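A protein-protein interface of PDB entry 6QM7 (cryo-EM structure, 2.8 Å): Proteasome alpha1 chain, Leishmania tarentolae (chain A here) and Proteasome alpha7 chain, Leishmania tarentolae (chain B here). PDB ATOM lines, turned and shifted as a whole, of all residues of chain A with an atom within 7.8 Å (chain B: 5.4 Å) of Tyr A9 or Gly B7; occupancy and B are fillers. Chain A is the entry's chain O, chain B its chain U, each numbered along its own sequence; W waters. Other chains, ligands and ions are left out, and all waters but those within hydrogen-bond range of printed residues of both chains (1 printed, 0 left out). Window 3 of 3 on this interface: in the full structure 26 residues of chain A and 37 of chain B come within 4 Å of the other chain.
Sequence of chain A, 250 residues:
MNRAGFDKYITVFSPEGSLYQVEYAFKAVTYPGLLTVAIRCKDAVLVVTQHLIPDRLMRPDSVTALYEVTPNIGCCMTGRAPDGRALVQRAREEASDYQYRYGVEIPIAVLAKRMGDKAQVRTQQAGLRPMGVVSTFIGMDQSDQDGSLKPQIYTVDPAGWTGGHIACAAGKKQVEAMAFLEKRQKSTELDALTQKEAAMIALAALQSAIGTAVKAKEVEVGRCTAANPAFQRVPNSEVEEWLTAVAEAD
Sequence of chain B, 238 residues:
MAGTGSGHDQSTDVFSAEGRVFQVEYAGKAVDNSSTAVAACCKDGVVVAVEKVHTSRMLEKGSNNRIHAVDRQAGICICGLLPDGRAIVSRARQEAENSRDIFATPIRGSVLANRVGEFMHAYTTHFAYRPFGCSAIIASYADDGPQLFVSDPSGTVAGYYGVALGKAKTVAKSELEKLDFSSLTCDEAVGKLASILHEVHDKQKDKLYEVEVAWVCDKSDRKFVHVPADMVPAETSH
Gly B7 touches Tyr A9 (C to CE1, 3.9 Å).
Tyr A9 touches His B8.
Tyr A9 touches Val B14 (O to CG2, 3.4 Å).
Gln A21 touches Asp B13 (OE1 to O, 3.7 Å).
CA of Val B14 touches OE1 of Gln A21, 3.4 Å away.
Gly A127 touches Asp B13 (O to CB, 3.2 Å).
Water W1 lies within hydrogen-bond range of N of Gly A127 (2.5 Å) and OD1 of Asp B13 (3.2 Å).
Tyr A9 touches three residues of chain B.
Printed residues of chain B within 4 Å of Gln A21: Asp B13 (3.7 Å) and Val B14 (3.4 Å).
Printed residues of chain B within 4 Å of Gly A127: Asp B13 (3.2 Å).
No residue of chain A comes within 4 Å of Ser B6.
Gly B7 touches just one residue of chain A: Tyr A9.
Of the printed residues of chain A, Asp B13 touches Gln A21 and Gly A127.
Of the printed residues of chain A, Val B14 touches Tyr A9 and Gln A21.
The nearest residue of chain B that does not touch Tyr A9 is Asp B13 (4.1 Å).
The side-chain amide nitrogen (NE2) of Gln A21 sits at hydrogen-bond distance from the backbone carbonyl oxygen (O) of Lys A8.
The backbone NH (N) of Ser B6 lies within hydrogen-bond range of a ring nitrogen (ND1) of His B8.
Hydrophobic or aromatic side chains of chain A that line the printed part of chain B: Tyr A9.
Along chain A the printed residues that touch a printed residue of chain B span positions 9 to 127.
Of the 8 printed residues of chain B, 4 touch a printed residue of chain A.
Printed residues of chain B that touch a printed residue of chain A: Gly B7, His B8, Asp B13 and Val B14.
Hydrophobic or aromatic side chains of chain B within 4 Å of the printed part of chain A: Val B14.
Among the printed residues, no Asp or Glu carboxylate lies within 4 Å of a Lys or Arg side-chain nitrogen of the other chain.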
ATOM      1  N   PHE A   6     -18.134   1.118  10.262  1.00  0.00           N
ATOM      2  CA  PHE A   6     -17.949  -0.279   9.748  1.00  0.00           C
ATOM      3  C   PHE A   6     -17.404  -1.184  10.862  1.00  0.00           C
ATOM      4  O   PHE A   6     -17.926  -2.296  11.048  1.00  0.00           O
ATOM      5  CB  PHE A   6     -17.019  -0.284   8.532  1.00  0.00           C
ATOM      6  CG  PHE A   6     -17.243  -1.437   7.586  1.00  0.00           C
ATOM      7  CD1 PHE A   6     -17.984  -1.267   6.421  1.00  0.00           C
ATOM      8  CD2 PHE A   6     -16.729  -2.696   7.863  1.00  0.00           C
ATOM      9  CE1 PHE A   6     -18.194  -2.327   5.551  1.00  0.00           C
ATOM     10  CE2 PHE A   6     -16.941  -3.757   6.992  1.00  0.00           C
ATOM     11  CZ  PHE A   6     -17.671  -3.569   5.837  1.00  0.00           C
ATOM     12  N   ASP A   7     -16.378  -0.707  11.575  1.00  0.00           N
ATOM     13  CA  ASP A   7     -15.808  -1.335  12.800  1.00  0.00           C
ATOM     14  C   ASP A   7     -16.878  -1.422  13.897  1.00  0.00           C
ATOM     15  O   ASP A   7     -16.784  -2.338  14.740  1.00  0.00           O
ATOM     16  CB  ASP A   7     -14.628  -0.528  13.361  1.00  0.00           C
ATOM     17  CG  ASP A   7     -13.450  -0.333  12.416  1.00  0.00           C
ATOM     18  OD1 ASP A   7     -12.969  -1.336  11.852  1.00  0.00           O
ATOM     19  OD2 ASP A   7     -13.011   0.826  12.268  1.00  0.00           O
ATOM     20  N   LYS A   8     -17.831  -0.479  13.898  1.00  0.00           N
ATOM     21  CA  LYS A   8     -18.671  -0.098  15.066  1.00  0.00           C
ATOM     22  C   LYS A   8     -19.992  -0.866  15.075  1.00  0.00           C
ATOM     23  O   LYS A   8     -20.663  -0.839  16.122  1.00  0.00           O
ATOM     24  CB  LYS A   8     -18.971   1.403  15.036  1.00  0.00           C
ATOM     25  CG  LYS A   8     -17.783   2.299  14.725  1.00  0.00           C
ATOM     26  CD  LYS A   8     -17.741   3.569  15.548  1.00  0.00           C
ATOM     27  CE  LYS A   8     -16.523   4.419  15.248  1.00  0.00           C
ATOM     28  NZ  LYS A   8     -15.900   4.935  16.489  1.00  0.00           N
ATOM     29  N   TYR A   9     -20.353  -1.504  13.960  1.00  0.00           N
ATOM     30  CA  TYR A   9     -21.698  -2.088  13.712  1.00  0.00           C
ATOM     31  C   TYR A   9     -21.625  -3.617  13.613  1.00  0.00           C
ATOM     32  O   TYR A   9     -22.629  -4.267  13.941  1.00  0.00           O
ATOM     33  CB  TYR A   9     -22.311  -1.466  12.457  1.00  0.00           C
ATOM     34  CG  TYR A   9     -22.188   0.037  12.352  1.00  0.00           C
ATOM     35  CD1 TYR A   9     -22.514   0.867  13.421  1.00  0.00           C
ATOM     36  CD2 TYR A   9     -21.760   0.632  11.171  1.00  0.00           C
ATOM     37  CE1 TYR A   9     -22.407   2.247  13.321  1.00  0.00           C
ATOM     38  CE2 TYR A   9     -21.652   2.010  11.053  1.00  0.00           C
ATOM     39  CZ  TYR A   9     -21.977   2.820  12.130  1.00  0.00           C
ATOM     40  OH  TYR A   9     -21.867   4.178  12.014  1.00  0.00           O
ATOM     41  N   ILE A  10     -20.503  -4.177  13.157  1.00  0.00           N
ATOM     42  CA  ILE A  10     -20.225  -5.641  13.269  1.00  0.00           C
ATOM     43  C   ILE A  10     -19.206  -5.855  14.385  1.00  0.00           C
ATOM     44  O   ILE A  10     -18.732  -4.873  14.990  1.00  0.00           O
ATOM     45  CB  ILE A  10     -19.767  -6.312  11.951  1.00  0.00           C
ATOM     46  CG1 ILE A  10     -18.897  -5.403  11.081  1.00  0.00           C
ATOM     47  CG2 ILE A  10     -20.965  -6.867  11.192  1.00  0.00           C
ATOM     48  CD1 ILE A  10     -18.181  -6.132   9.958  1.00  0.00           C
ATOM     49  N   THR A  11     -18.936  -7.127  14.655  1.00  0.00           N
ATOM     50  CA  THR A  11     -18.011  -7.599  15.702  1.00  0.00           C
ATOM     51  C   THR A  11     -16.674  -7.867  15.004  1.00  0.00           C
ATOM     52  O   THR A  11     -16.368  -9.019  14.655  1.00  0.00           O
ATOM     53  CB  THR A  11     -18.725  -8.704  16.495  1.00  0.00           C
ATOM     54  OG1 THR A  11     -18.232  -8.625  17.836  1.00  0.00           O
ATOM     55  CG2 THR A  11     -18.594 -10.087  15.884  1.00  0.00           C
ATOM     56  N   VAL A  12     -15.951  -6.785  14.738  1.00  0.00           N
ATOM     57  CA  VAL A  12     -14.572  -6.801  14.184  1.00  0.00           C
ATOM     58  C   VAL A  12     -13.731  -5.817  14.990  1.00  0.00           C
ATOM     59  O   VAL A  12     -14.291  -4.843  15.548  1.00  0.00           O
ATOM     60  CB  VAL A  12     -14.544  -6.446  12.688  1.00  0.00           C
ATOM     61  CG1 VAL A  12     -15.262  -7.487  11.856  1.00  0.00           C
ATOM     62  CG2 VAL A  12     -15.100  -5.065  12.412  1.00  0.00           C
ATOM     63  N   TYR A  20     -15.991  -2.511  19.336  1.00  0.00           N
ATOM     64  CA  TYR A  20     -16.870  -1.377  19.716  1.00  0.00           C
ATOM     65  C   TYR A  20     -18.220  -1.917  20.197  1.00  0.00           C
ATOM     66  O   TYR A  20     -18.738  -1.383  21.178  1.00  0.00           O
ATOM     67  CB  TYR A  20     -17.002  -0.363  18.576  1.00  0.00           C
ATOM     68  CG  TYR A  20     -15.867   0.628  18.489  1.00  0.00           C
ATOM     69  CD1 TYR A  20     -15.552   1.452  19.560  1.00  0.00           C
ATOM     70  CD2 TYR A  20     -15.108   0.750  17.335  1.00  0.00           C
ATOM     71  CE1 TYR A  20     -14.508   2.363  19.494  1.00  0.00           C
ATOM     72  CE2 TYR A  20     -14.071   1.667  17.245  1.00  0.00           C
ATOM     73  CZ  TYR A  20     -13.762   2.471  18.332  1.00  0.00           C
ATOM     74  OH  TYR A  20     -12.733   3.365  18.251  1.00  0.00           O
ATOM     75  N   GLN A  21     -18.757  -2.957  19.565  1.00  0.00           N
ATOM     76  CA  GLN A  21     -20.103  -3.485  19.907  1.00  0.00           C
ATOM     77  C   GLN A  21     -20.114  -4.029  21.338  1.00  0.00           C
ATOM     78  O   GLN A  21     -21.166  -3.924  21.992  1.00  0.00           O
ATOM     79  CB  GLN A  21     -20.563  -4.552  18.912  1.00  0.00           C
ATOM     80  CG  GLN A  21     -21.191  -3.961  17.657  1.00  0.00           C
ATOM     81  CD  GLN A  21     -22.505  -3.295  17.973  1.00  0.00           C
ATOM     82  OE1 GLN A  21     -23.466  -3.959  18.353  1.00  0.00           O
ATOM     83  NE2 GLN A  21     -22.534  -1.976  17.861  1.00  0.00           N
ATOM     84  N   TYR A  24     -20.041  -1.035  23.738  1.00  0.00           N
ATOM     85  CA  TYR A  24     -21.403  -0.463  23.698  1.00  0.00           C
ATOM     86  C   TYR A  24     -22.367  -1.327  24.508  1.00  0.00           C
ATOM     87  O   TYR A  24     -23.256  -0.748  25.130  1.00  0.00           O
ATOM     88  CB  TYR A  24     -21.878  -0.294  22.256  1.00  0.00           C
ATOM     89  CG  TYR A  24     -21.126   0.714  21.420  1.00  0.00           C
ATOM     90  CD1 TYR A  24     -20.212   1.608  21.969  1.00  0.00           C
ATOM     91  CD2 TYR A  24     -21.352   0.785  20.051  1.00  0.00           C
ATOM     92  CE1 TYR A  24     -19.527   2.520  21.180  1.00  0.00           C
ATOM     93  CE2 TYR A  24     -20.690   1.706  19.252  1.00  0.00           C
ATOM     94  CZ  TYR A  24     -19.771   2.575  19.817  1.00  0.00           C
ATOM     95  OH  TYR A  24     -19.121   3.478  19.025  1.00  0.00           O
ATOM     96  N   ALA A 126     -20.299 -12.572  13.789  1.00  0.00           N
ATOM     97  CA  ALA A 126     -21.077 -11.400  13.329  1.00  0.00           C
ATOM     98  C   ALA A 126     -22.570 -11.741  13.366  1.00  0.00           C
ATOM     99  O   ALA A 126     -22.934 -12.932  13.193  1.00  0.00           O
ATOM    100  CB  ALA A 126     -20.657 -10.958  11.946  1.00  0.00           C
ATOM    101  N   GLY A 127     -23.385 -10.719  13.634  1.00  0.00           N
ATOM    102  CA  GLY A 127     -24.841 -10.721  13.424  1.00  0.00           C
ATOM    103  C   GLY A 127     -25.609 -11.078  14.675  1.00  0.00           C
ATOM    104  O   GLY A 127     -26.824 -10.854  14.688  1.00  0.00           O
ATOM    105  N   LEU A 128     -24.950 -11.670  15.665  1.00  0.00           N
ATOM    106  CA  LEU A 128     -25.514 -11.884  17.018  1.00  0.00           C
ATOM    107  C   LEU A 128     -25.190 -10.637  17.836  1.00  0.00           C
ATOM    108  O   LEU A 128     -24.010 -10.246  17.857  1.00  0.00           O
ATOM    109  CB  LEU A 128     -24.892 -13.141  17.634  1.00  0.00           C
ATOM    110  CG  LEU A 128     -25.066 -14.413  16.804  1.00  0.00           C
ATOM    111  CD1 LEU A 128     -24.317 -15.596  17.420  1.00  0.00           C
ATOM    112  CD2 LEU A 128     -26.554 -14.718  16.619  1.00  0.00           C
ATOM    113  N   PRO A 130     -24.465  -8.808  21.308  1.00  0.00           N
ATOM    114  CA  PRO A 130     -24.165  -9.105  22.703  1.00  0.00           C
ATOM    115  C   PRO A 130     -25.379  -8.894  23.612  1.00  0.00           C
ATOM    116  O   PRO A 130     -26.150  -7.998  23.387  1.00  0.00           O
ATOM    117  CB  PRO A 130     -23.073  -8.088  23.034  1.00  0.00           C
ATOM    118  CG  PRO A 130     -22.375  -7.897  21.714  1.00  0.00           C
ATOM    119  CD  PRO A 130     -23.511  -7.867  20.715  1.00  0.00           C
ATOM    120  N   SER B   6     -25.568   6.637  10.505  1.00  0.00           N
ATOM    121  CA  SER B   6     -26.590   6.044   9.575  1.00  0.00           C
ATOM    122  C   SER B   6     -26.710   4.525   9.787  1.00  0.00           C
ATOM    123  O   SER B   6     -27.852   4.025   9.761  1.00  0.00           O
ATOM    124  CB  SER B   6     -26.283   6.379   8.128  1.00  0.00           C
ATOM    125  OG  SER B   6     -24.953   6.017   7.785  1.00  0.00           O
ATOM    126  N   GLY B   7     -25.584   3.825   9.984  1.00  0.00           N
ATOM    127  CA  GLY B   7     -25.515   2.355  10.129  1.00  0.00           C
ATOM    128  C   GLY B   7     -25.845   1.873  11.535  1.00  0.00           C
ATOM    129  O   GLY B   7     -26.070   0.653  11.692  1.00  0.00           O
ATOM    130  N   HIS B   8     -25.873   2.780  12.520  1.00  0.00           N
ATOM    131  CA  HIS B   8     -26.115   2.478  13.961  1.00  0.00           C
ATOM    132  C   HIS B   8     -27.507   1.872  14.196  1.00  0.00           C
ATOM    133  O   HIS B   8     -27.639   1.173  15.215  1.00  0.00           O
ATOM    134  CB  HIS B   8     -25.842   3.712  14.852  1.00  0.00           C
ATOM    135  CG  HIS B   8     -26.747   4.888  14.654  1.00  0.00           C
ATOM    136  ND1 HIS B   8     -27.019   5.427  13.403  1.00  0.00           N
ATOM    137  CD2 HIS B   8     -27.399   5.670  15.546  1.00  0.00           C
ATOM    138  CE1 HIS B   8     -27.824   6.466  13.532  1.00  0.00           C
ATOM    139  NE2 HIS B   8     -28.075   6.633  14.839  1.00  0.00           N
ATOM    140  N   ASP B   9     -28.488   2.094  13.303  1.00  0.00           N
ATOM    141  CA  ASP B   9     -29.934   1.832  13.559  1.00  0.00           C
ATOM    142  C   ASP B   9     -30.594   0.980  12.465  1.00  0.00           C
ATOM    143  O   ASP B   9     -31.840   0.903  12.463  1.00  0.00           O
ATOM    144  CB  ASP B   9     -30.679   3.159  13.708  1.00  0.00           C
ATOM    145  CG  ASP B   9     -30.868   3.933  12.415  1.00  0.00           C
ATOM    146  OD1 ASP B   9     -31.612   4.943  12.450  1.00  0.00           O
ATOM    147  OD2 ASP B   9     -30.282   3.520  11.385  1.00  0.00           O
ATOM    148  N   GLN B  10     -29.821   0.372  11.566  1.00  0.00           N
ATOM    149  CA  GLN B  10     -30.371  -0.339  10.380  1.00  0.00           C
ATOM    150  C   GLN B  10     -30.873  -1.721  10.785  1.00  0.00           C
ATOM    151  O   GLN B  10     -31.819  -2.213  10.133  1.00  0.00           O
ATOM    152  CB  GLN B  10     -29.333  -0.472   9.263  1.00  0.00           C
ATOM    153  CG  GLN B  10     -29.072   0.828   8.517  1.00  0.00           C
ATOM    154  CD  GLN B  10     -30.324   1.384   7.889  1.00  0.00           C
ATOM    155  OE1 GLN B  10     -31.083   0.666   7.243  1.00  0.00           O
ATOM    156  NE2 GLN B  10     -30.552   2.670   8.100  1.00  0.00           N
ATOM    157  N   SER B  11     -30.247  -2.337  11.786  1.00  0.00           N
ATOM    158  CA  SER B  11     -30.637  -3.676  12.280  1.00  0.00           C
ATOM    159  C   SER B  11     -30.565  -3.726  13.802  1.00  0.00           C
ATOM    160  O   SER B  11     -29.875  -2.906  14.428  1.00  0.00           O
ATOM    161  CB  SER B  11     -29.813  -4.766  11.655  1.00  0.00           C
ATOM    162  OG  SER B  11     -28.556  -4.867  12.303  1.00  0.00           O
ATOM    163  N   ASP B  13     -29.360  -6.107  15.573  1.00  0.00           N
ATOM    164  CA  ASP B  13     -28.174  -6.841  16.084  1.00  0.00           C
ATOM    165  C   ASP B  13     -27.120  -5.852  16.574  1.00  0.00           C
ATOM    166  O   ASP B  13     -26.049  -6.303  17.007  1.00  0.00           O
ATOM    167  CB  ASP B  13     -27.601  -7.801  15.042  1.00  0.00           C
ATOM    168  CG  ASP B  13     -26.639  -7.192  14.031  1.00  0.00           C
ATOM    169  OD1 ASP B  13     -25.405  -7.333  14.239  1.00  0.00           O
ATOM    170  OD2 ASP B  13     -27.119  -6.621  13.024  1.00  0.00           O
ATOM    171  N   VAL B  14     -27.404  -4.560  16.510  1.00  0.00           N
ATOM    172  CA  VAL B  14     -26.386  -3.492  16.669  1.00  0.00           C
ATOM    173  C   VAL B  14     -26.809  -2.598  17.823  1.00  0.00           C
ATOM    174  O   VAL B  14     -27.849  -1.929  17.688  1.00  0.00           O
ATOM    175  CB  VAL B  14     -26.244  -2.666  15.378  1.00  0.00           C
ATOM    176  CG1 VAL B  14     -25.205  -1.565  15.540  1.00  0.00           C
ATOM    177  CG2 VAL B  14     -25.923  -3.552  14.184  1.00  0.00           C
HETATM  178  O   HOH W   1     -22.479  -8.524  14.310  1.00  0.00           O
